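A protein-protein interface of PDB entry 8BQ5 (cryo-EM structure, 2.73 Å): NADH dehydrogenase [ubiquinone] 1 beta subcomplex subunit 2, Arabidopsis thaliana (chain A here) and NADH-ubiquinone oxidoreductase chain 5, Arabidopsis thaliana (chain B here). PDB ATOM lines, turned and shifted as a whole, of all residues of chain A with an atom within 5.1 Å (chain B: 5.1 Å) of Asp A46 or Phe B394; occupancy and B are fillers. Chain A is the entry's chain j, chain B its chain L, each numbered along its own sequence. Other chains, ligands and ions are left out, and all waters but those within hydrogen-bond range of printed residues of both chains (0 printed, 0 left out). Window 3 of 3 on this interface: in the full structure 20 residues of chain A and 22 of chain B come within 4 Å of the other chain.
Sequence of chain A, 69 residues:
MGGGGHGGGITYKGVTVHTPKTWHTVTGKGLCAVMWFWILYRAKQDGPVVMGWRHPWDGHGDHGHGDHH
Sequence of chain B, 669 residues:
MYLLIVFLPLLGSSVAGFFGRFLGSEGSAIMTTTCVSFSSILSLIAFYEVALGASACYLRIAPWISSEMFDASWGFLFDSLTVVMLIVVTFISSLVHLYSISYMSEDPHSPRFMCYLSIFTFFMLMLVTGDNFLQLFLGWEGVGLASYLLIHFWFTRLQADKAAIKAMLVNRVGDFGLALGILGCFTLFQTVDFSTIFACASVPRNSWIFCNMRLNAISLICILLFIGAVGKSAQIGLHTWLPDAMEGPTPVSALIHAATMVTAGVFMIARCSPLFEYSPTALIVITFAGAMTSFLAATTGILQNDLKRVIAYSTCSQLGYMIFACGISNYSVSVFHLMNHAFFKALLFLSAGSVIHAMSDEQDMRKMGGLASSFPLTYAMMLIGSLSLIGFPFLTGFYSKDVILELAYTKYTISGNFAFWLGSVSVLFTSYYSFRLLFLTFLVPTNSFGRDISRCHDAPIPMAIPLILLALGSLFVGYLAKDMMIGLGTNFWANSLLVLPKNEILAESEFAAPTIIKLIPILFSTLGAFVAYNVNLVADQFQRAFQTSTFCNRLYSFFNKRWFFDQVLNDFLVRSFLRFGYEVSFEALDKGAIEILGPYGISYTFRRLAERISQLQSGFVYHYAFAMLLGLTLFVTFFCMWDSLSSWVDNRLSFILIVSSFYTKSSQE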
ATOM      1  N   TRP A  38      16.887  25.845  -6.017  1.00  0.00           N
ATOM      2  CA  TRP A  38      18.164  25.271  -5.607  1.00  0.00           C
ATOM      3  C   TRP A  38      19.122  26.348  -5.117  1.00  0.00           C
ATOM      4  O   TRP A  38      19.791  26.177  -4.091  1.00  0.00           O
ATOM      5  CB  TRP A  38      18.779  24.497  -6.773  1.00  0.00           C
ATOM      6  CG  TRP A  38      20.122  23.897  -6.488  1.00  0.00           C
ATOM      7  CD1 TRP A  38      21.317  24.283  -7.020  1.00  0.00           C
ATOM      8  CD2 TRP A  38      20.407  22.788  -5.627  1.00  0.00           C
ATOM      9  NE1 TRP A  38      22.329  23.494  -6.536  1.00  0.00           N
ATOM     10  CE2 TRP A  38      21.797  22.567  -5.678  1.00  0.00           C
ATOM     11  CE3 TRP A  38      19.624  21.966  -4.813  1.00  0.00           C
ATOM     12  CZ2 TRP A  38      22.421  21.559  -4.949  1.00  0.00           C
ATOM     13  CZ3 TRP A  38      20.245  20.964  -4.089  1.00  0.00           C
ATOM     14  CH2 TRP A  38      21.629  20.770  -4.160  1.00  0.00           C
ATOM     15  N   ILE A  39      19.195  27.470  -5.833  1.00  0.00           N
ATOM     16  CA  ILE A  39      20.156  28.514  -5.487  1.00  0.00           C
ATOM     17  C   ILE A  39      19.765  29.196  -4.183  1.00  0.00           C
ATOM     18  O   ILE A  39      20.618  29.480  -3.334  1.00  0.00           O
ATOM     19  CB  ILE A  39      20.287  29.517  -6.648  1.00  0.00           C
ATOM     20  CG1 ILE A  39      21.000  28.857  -7.830  1.00  0.00           C
ATOM     21  CG2 ILE A  39      21.039  30.760  -6.209  1.00  0.00           C
ATOM     22  CD1 ILE A  39      20.917  29.647  -9.111  1.00  0.00           C
ATOM     23  N   ARG A  42      20.572  26.828  -1.305  1.00  0.00           N
ATOM     24  CA  ARG A  42      22.025  26.660  -1.044  1.00  0.00           C
ATOM     25  C   ARG A  42      22.580  27.991  -0.528  1.00  0.00           C
ATOM     26  O   ARG A  42      23.510  27.950   0.273  1.00  0.00           O
ATOM     27  CB  ARG A  42      22.773  26.147  -2.276  1.00  0.00           C
ATOM     28  CG  ARG A  42      22.476  24.697  -2.625  1.00  0.00           C
ATOM     29  CD  ARG A  42      23.600  23.765  -2.219  1.00  0.00           C
ATOM     30  NE  ARG A  42      23.647  23.561  -0.779  1.00  0.00           N
ATOM     31  CZ  ARG A  42      22.970  22.626  -0.122  1.00  0.00           C
ATOM     32  NH1 ARG A  42      22.189  21.781  -0.774  1.00  0.00           N
ATOM     33  NH2 ARG A  42      23.084  22.535   1.191  1.00  0.00           N
ATOM     34  N   ALA A  43      22.012  29.122  -0.947  1.00  0.00           N
ATOM     35  CA  ALA A  43      22.437  30.419  -0.372  1.00  0.00           C
ATOM     36  C   ALA A  43      21.999  30.470   1.095  1.00  0.00           C
ATOM     37  O   ALA A  43      22.740  31.037   1.903  1.00  0.00           O
ATOM     38  CB  ALA A  43      21.856  31.558  -1.164  1.00  0.00           C
ATOM     39  N   LYS A  44      20.836  29.891   1.424  1.00  0.00           N
ATOM     40  CA  LYS A  44      20.388  29.822   2.838  1.00  0.00           C
ATOM     41  C   LYS A  44      21.411  29.055   3.677  1.00  0.00           C
ATOM     42  O   LYS A  44      21.735  29.546   4.772  1.00  0.00           O
ATOM     43  CB  LYS A  44      19.036  29.112   2.963  1.00  0.00           C
ATOM     44  CG  LYS A  44      18.229  29.455   4.209  1.00  0.00           C
ATOM     45  CD  LYS A  44      17.838  28.239   5.020  1.00  0.00           C
ATOM     46  CE  LYS A  44      16.696  27.458   4.407  1.00  0.00           C
ATOM     47  NZ  LYS A  44      16.355  26.265   5.216  1.00  0.00           N
ATOM     48  N   GLN A  45      21.922  27.919   3.184  1.00  0.00           N
ATOM     49  CA  GLN A  45      22.808  27.077   4.035  1.00  0.00           C
ATOM     50  C   GLN A  45      24.291  27.452   3.911  1.00  0.00           C
ATOM     51  O   GLN A  45      24.982  27.382   4.947  1.00  0.00           O
ATOM     52  CB  GLN A  45      22.627  25.596   3.695  1.00  0.00           C
ATOM     53  CG  GLN A  45      21.246  25.041   4.012  1.00  0.00           C
ATOM     54  CD  GLN A  45      20.249  25.279   2.905  1.00  0.00           C
ATOM     55  OE1 GLN A  45      20.566  25.866   1.873  1.00  0.00           O
ATOM     56  NE2 GLN A  45      19.024  24.827   3.119  1.00  0.00           N
ATOM     57  N   ASP A  46      24.764  27.837   2.723  1.00  0.00           N
ATOM     58  CA  ASP A  46      26.224  28.060   2.522  1.00  0.00           C
ATOM     59  C   ASP A  46      26.557  29.544   2.354  1.00  0.00           C
ATOM     60  O   ASP A  46      27.732  29.876   2.482  1.00  0.00           O
ATOM     61  CB  ASP A  46      26.769  27.255   1.338  1.00  0.00           C
ATOM     62  CG  ASP A  46      26.857  25.750   1.548  1.00  0.00           C
ATOM     63  OD1 ASP A  46      26.764  25.322   2.712  1.00  0.00           O
ATOM     64  OD2 ASP A  46      26.995  25.017   0.550  1.00  0.00           O
ATOM     65  N   GLY A  47      25.577  30.394   2.057  1.00  0.00           N
ATOM     66  CA  GLY A  47      25.837  31.846   1.985  1.00  0.00           C
ATOM     67  C   GLY A  47      26.602  32.330   3.202  1.00  0.00           C
ATOM     68  O   GLY A  47      27.698  32.863   3.003  1.00  0.00           O
ATOM     69  N   PRO A  48      26.106  32.162   4.454  1.00  0.00           N
ATOM     70  CA  PRO A  48      26.888  32.509   5.647  1.00  0.00           C
ATOM     71  C   PRO A  48      28.309  31.919   5.631  1.00  0.00           C
ATOM     72  O   PRO A  48      29.228  32.667   5.878  1.00  0.00           O
ATOM     73  CB  PRO A  48      26.082  31.914   6.811  1.00  0.00           C
ATOM     74  CG  PRO A  48      25.060  31.009   6.152  1.00  0.00           C
ATOM     75  CD  PRO A  48      24.777  31.674   4.823  1.00  0.00           C
ATOM     76  N   VAL A  49      28.451  30.620   5.337  1.00  0.00           N
ATOM     77  CA  VAL A  49      29.786  29.941   5.339  1.00  0.00           C
ATOM     78  C   VAL A  49      30.729  30.590   4.315  1.00  0.00           C
ATOM     79  O   VAL A  49      31.845  30.962   4.718  1.00  0.00           O
ATOM     80  CB  VAL A  49      29.671  28.427   5.080  1.00  0.00           C
ATOM     81  CG1 VAL A  49      30.895  27.674   5.574  1.00  0.00           C
ATOM     82  CG2 VAL A  49      28.404  27.831   5.666  1.00  0.00           C
ATOM     83  N   VAL A  50      30.315  30.699   3.044  1.00  0.00           N
ATOM     84  CA  VAL A  50      31.220  31.238   1.981  1.00  0.00           C
ATOM     85  C   VAL A  50      31.449  32.736   2.221  1.00  0.00           C
ATOM     86  O   VAL A  50      32.577  33.203   1.960  1.00  0.00           O
ATOM     87  CB  VAL A  50      30.707  30.926   0.558  1.00  0.00           C
ATOM     88  CG1 VAL A  50      29.470  31.718   0.156  1.00  0.00           C
ATOM     89  CG2 VAL A  50      31.799  31.060  -0.492  1.00  0.00           C
ATOM     90  N   MET A  51      30.442  33.448   2.738  1.00  0.00           N
ATOM     91  CA  MET A  51      30.622  34.887   3.064  1.00  0.00           C
ATOM     92  C   MET A  51      31.589  35.005   4.242  1.00  0.00           C
ATOM     93  O   MET A  51      31.982  36.142   4.535  1.00  0.00           O
ATOM     94  CB  MET A  51      29.295  35.574   3.388  1.00  0.00           C
ATOM     95  CG  MET A  51      28.941  36.681   2.420  1.00  0.00           C
ATOM     96  SD  MET A  51      28.331  36.042   0.840  1.00  0.00           S
ATOM     97  CE  MET A  51      26.591  35.843   1.220  1.00  0.00           C
ATOM     98  N   PHE B 392      28.161  30.816 -11.763  1.00  0.00           N
ATOM     99  CA  PHE B 392      27.104  31.294 -10.889  1.00  0.00           C
ATOM    100  C   PHE B 392      27.026  30.397  -9.657  1.00  0.00           C
ATOM    101  O   PHE B 392      27.138  29.171  -9.776  1.00  0.00           O
ATOM    102  CB  PHE B 392      25.764  31.315 -11.627  1.00  0.00           C
ATOM    103  CG  PHE B 392      24.736  32.201 -10.990  1.00  0.00           C
ATOM    104  CD1 PHE B 392      23.827  31.689 -10.080  1.00  0.00           C
ATOM    105  CD2 PHE B 392      24.681  33.551 -11.296  1.00  0.00           C
ATOM    106  CE1 PHE B 392      22.883  32.505  -9.493  1.00  0.00           C
ATOM    107  CE2 PHE B 392      23.737  34.371 -10.712  1.00  0.00           C
ATOM    108  CZ  PHE B 392      22.837  33.847  -9.809  1.00  0.00           C
ATOM    109  N   PRO B 393      26.846  30.968  -8.466  1.00  0.00           N
ATOM    110  CA  PRO B 393      27.013  30.190  -7.233  1.00  0.00           C
ATOM    111  C   PRO B 393      26.110  28.967  -7.169  1.00  0.00           C
ATOM    112  O   PRO B 393      24.957  28.994  -7.606  1.00  0.00           O
ATOM    113  CB  PRO B 393      26.661  31.200  -6.139  1.00  0.00           C
ATOM    114  CG  PRO B 393      27.030  32.514  -6.716  1.00  0.00           C
ATOM    115  CD  PRO B 393      26.806  32.417  -8.205  1.00  0.00           C
ATOM    116  N   PHE B 394      26.662  27.881  -6.629  1.00  0.00           N
ATOM    117  CA  PHE B 394      25.982  26.640  -6.276  1.00  0.00           C
ATOM    118  C   PHE B 394      25.475  25.863  -7.483  1.00  0.00           C
ATOM    119  O   PHE B 394      24.795  24.846  -7.304  1.00  0.00           O
ATOM    120  CB  PHE B 394      24.824  26.884  -5.299  1.00  0.00           C
ATOM    121  CG  PHE B 394      25.169  27.844  -4.197  1.00  0.00           C
ATOM    122  CD1 PHE B 394      26.149  27.533  -3.271  1.00  0.00           C
ATOM    123  CD2 PHE B 394      24.533  29.069  -4.105  1.00  0.00           C
ATOM    124  CE1 PHE B 394      26.477  28.419  -2.265  1.00  0.00           C
ATOM    125  CE2 PHE B 394      24.856  29.959  -3.103  1.00  0.00           C
ATOM    126  CZ  PHE B 394      25.829  29.632  -2.180  1.00  0.00           C
ATOM    127  N   LEU B 395      25.774  26.300  -8.702  1.00  0.00           N
ATOM    128  CA  LEU B 395      25.543  25.469  -9.869  1.00  0.00           C
ATOM    129  C   LEU B 395      26.749  24.558 -10.092  1.00  0.00           C
ATOM    130  O   LEU B 395      27.695  24.537  -9.302  1.00  0.00           O
ATOM    131  CB  LEU B 395      25.268  26.335 -11.096  1.00  0.00           C
ATOM    132  CG  LEU B 395      24.102  27.313 -10.934  1.00  0.00           C
ATOM    133  CD1 LEU B 395      23.849  28.073 -12.221  1.00  0.00           C
ATOM    134  CD2 LEU B 395      22.848  26.585 -10.480  1.00  0.00           C
ATOM    135  N   THR B 396      26.708  23.787 -11.182  1.00  0.00           N
ATOM    136  CA  THR B 396      27.776  22.822 -11.430  1.00  0.00           C
ATOM    137  C   THR B 396      29.119  23.516 -11.635  1.00  0.00           C
ATOM    138  O   THR B 396      30.152  23.040 -11.150  1.00  0.00           O
ATOM    139  CB  THR B 396      27.425  21.941 -12.631  1.00  0.00           C
ATOM    140  OG1 THR B 396      26.507  20.921 -12.220  1.00  0.00           O
ATOM    141  CG2 THR B 396      28.663  21.278 -13.202  1.00  0.00           C
ATOM    142  N   PHE B 398      30.253  26.388 -10.356  1.00  0.00           N
ATOM    143  CA  PHE B 398      30.809  27.143  -9.203  1.00  0.00           C
ATOM    144  C   PHE B 398      31.723  26.278  -8.347  1.00  0.00           C
ATOM    145  O   PHE B 398      32.710  26.822  -7.828  1.00  0.00           O
ATOM    146  CB  PHE B 398      29.662  27.663  -8.331  1.00  0.00           C
ATOM    147  CG  PHE B 398      30.042  28.197  -6.974  1.00  0.00           C
ATOM    148  CD1 PHE B 398      30.558  29.474  -6.834  1.00  0.00           C
ATOM    149  CD2 PHE B 398      29.851  27.432  -5.832  1.00  0.00           C
ATOM    150  CE1 PHE B 398      30.898  29.965  -5.583  1.00  0.00           C
ATOM    151  CE2 PHE B 398      30.194  27.924  -4.584  1.00  0.00           C
ATOM    152  CZ  PHE B 398      30.715  29.190  -4.462  1.00  0.00           C
ATOM    153  N   TYR B 399      31.464  24.972  -8.252  1.00  0.00           N
ATOM    154  CA  TYR B 399      32.217  24.202  -7.268  1.00  0.00           C
ATOM    155  C   TYR B 399      33.634  23.869  -7.719  1.00  0.00           C
ATOM    156  O   TYR B 399      34.477  23.557  -6.873  1.00  0.00           O
ATOM    157  CB  TYR B 399      31.461  22.919  -6.924  1.00  0.00           C
ATOM    158  CG  TYR B 399      30.302  23.148  -5.982  1.00  0.00           C
ATOM    159  CD1 TYR B 399      28.998  23.198  -6.452  1.00  0.00           C
ATOM    160  CD2 TYR B 399      30.516  23.349  -4.626  1.00  0.00           C
ATOM    161  CE1 TYR B 399      27.937  23.416  -5.593  1.00  0.00           C
ATOM    162  CE2 TYR B 399      29.463  23.568  -3.760  1.00  0.00           C
ATOM    163  CZ  TYR B 399      28.176  23.601  -4.249  1.00  0.00           C
ATOM    164  OH  TYR B 399      27.122  23.821  -3.391  1.00  0.00           O
ATOM    165  N   LEU B 475      23.128  21.301 -12.814  1.00  0.00           N
ATOM    166  CA  LEU B 475      22.614  21.943 -11.613  1.00  0.00           C
ATOM    167  C   LEU B 475      23.058  21.232 -10.342  1.00  0.00           C
ATOM    168  O   LEU B 475      23.196  21.868  -9.293  1.00  0.00           O
ATOM    169  CB  LEU B 475      21.084  21.999 -11.663  1.00  0.00           C
ATOM    170  CG  LEU B 475      20.479  22.882 -12.752  1.00  0.00           C
ATOM    171  CD1 LEU B 475      18.986  22.645 -12.891  1.00  0.00           C
ATOM    172  CD2 LEU B 475      20.759  24.331 -12.440  1.00  0.00           C
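O of Phe B394 is in hydrogen-bond range of NE1 of Trp A38, 2.9 Å away.
The indole nitrogen (NE1) of Trp A38 sits at hydrogen-bond distance from the backbone carbonyl oxygen (O) of Leu B475 (3.3 Å).
N of Leu B475 lies within hydrogen-bond range of OG1 of Thr B396, 3.5 Å away.
N of Arg A42 lies within hydrogen-bond range of OE1 of Gln A45, 3.3 Å away.
OD2 of Asp A46 is in salt-bridge range of NE of Arg A42 (3.9 Å).
Among the printed residues, merely in contact across the chains: Ile A39 with Phe B392 (3.5 Å), Ile A39 with Pro B393 (3.97 Å), Ile A39 with Leu B395 (3.9 Å), Arg A42 with Phe B394 (3.5 Å), Arg A42 with Tyr B399 (3.7 Å), Ala A43 with Phe B394 (3.7 Å) and Asp A46 with Phe B394 (3.8 Å).
Printed residues of chain B within 4 Å of Ile A39: Phe B392, Pro B393 and Leu B395.
Of the printed residues of chain B, Arg A42 touches Phe B394 and Tyr B399.
Of chain B, only Phe B394 (3.8 Å) comes within 4 Å of Asp A46.
Gly A47 touches none of the printed residues of chain B.
Met A51 touches none of the printed residues of chain B.
Of the printed residues of chain A, Phe B394 touches Trp A38 (2.9 Å), Arg A42 (3.5 Å), Ala A43 (3.7 Å) and Asp A46 (3.8 Å).
Of the printed residues of chain A, Tyr B399 touches Arg A42.
The nearest printed residue of chain A that does not touch Tyr B399 is Asp A46 (4.1 Å).
Among the printed residues, no Asp or Glu carboxylate lies within 4 Å of a Lys or Arg side-chain nitrogen of the other chain.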
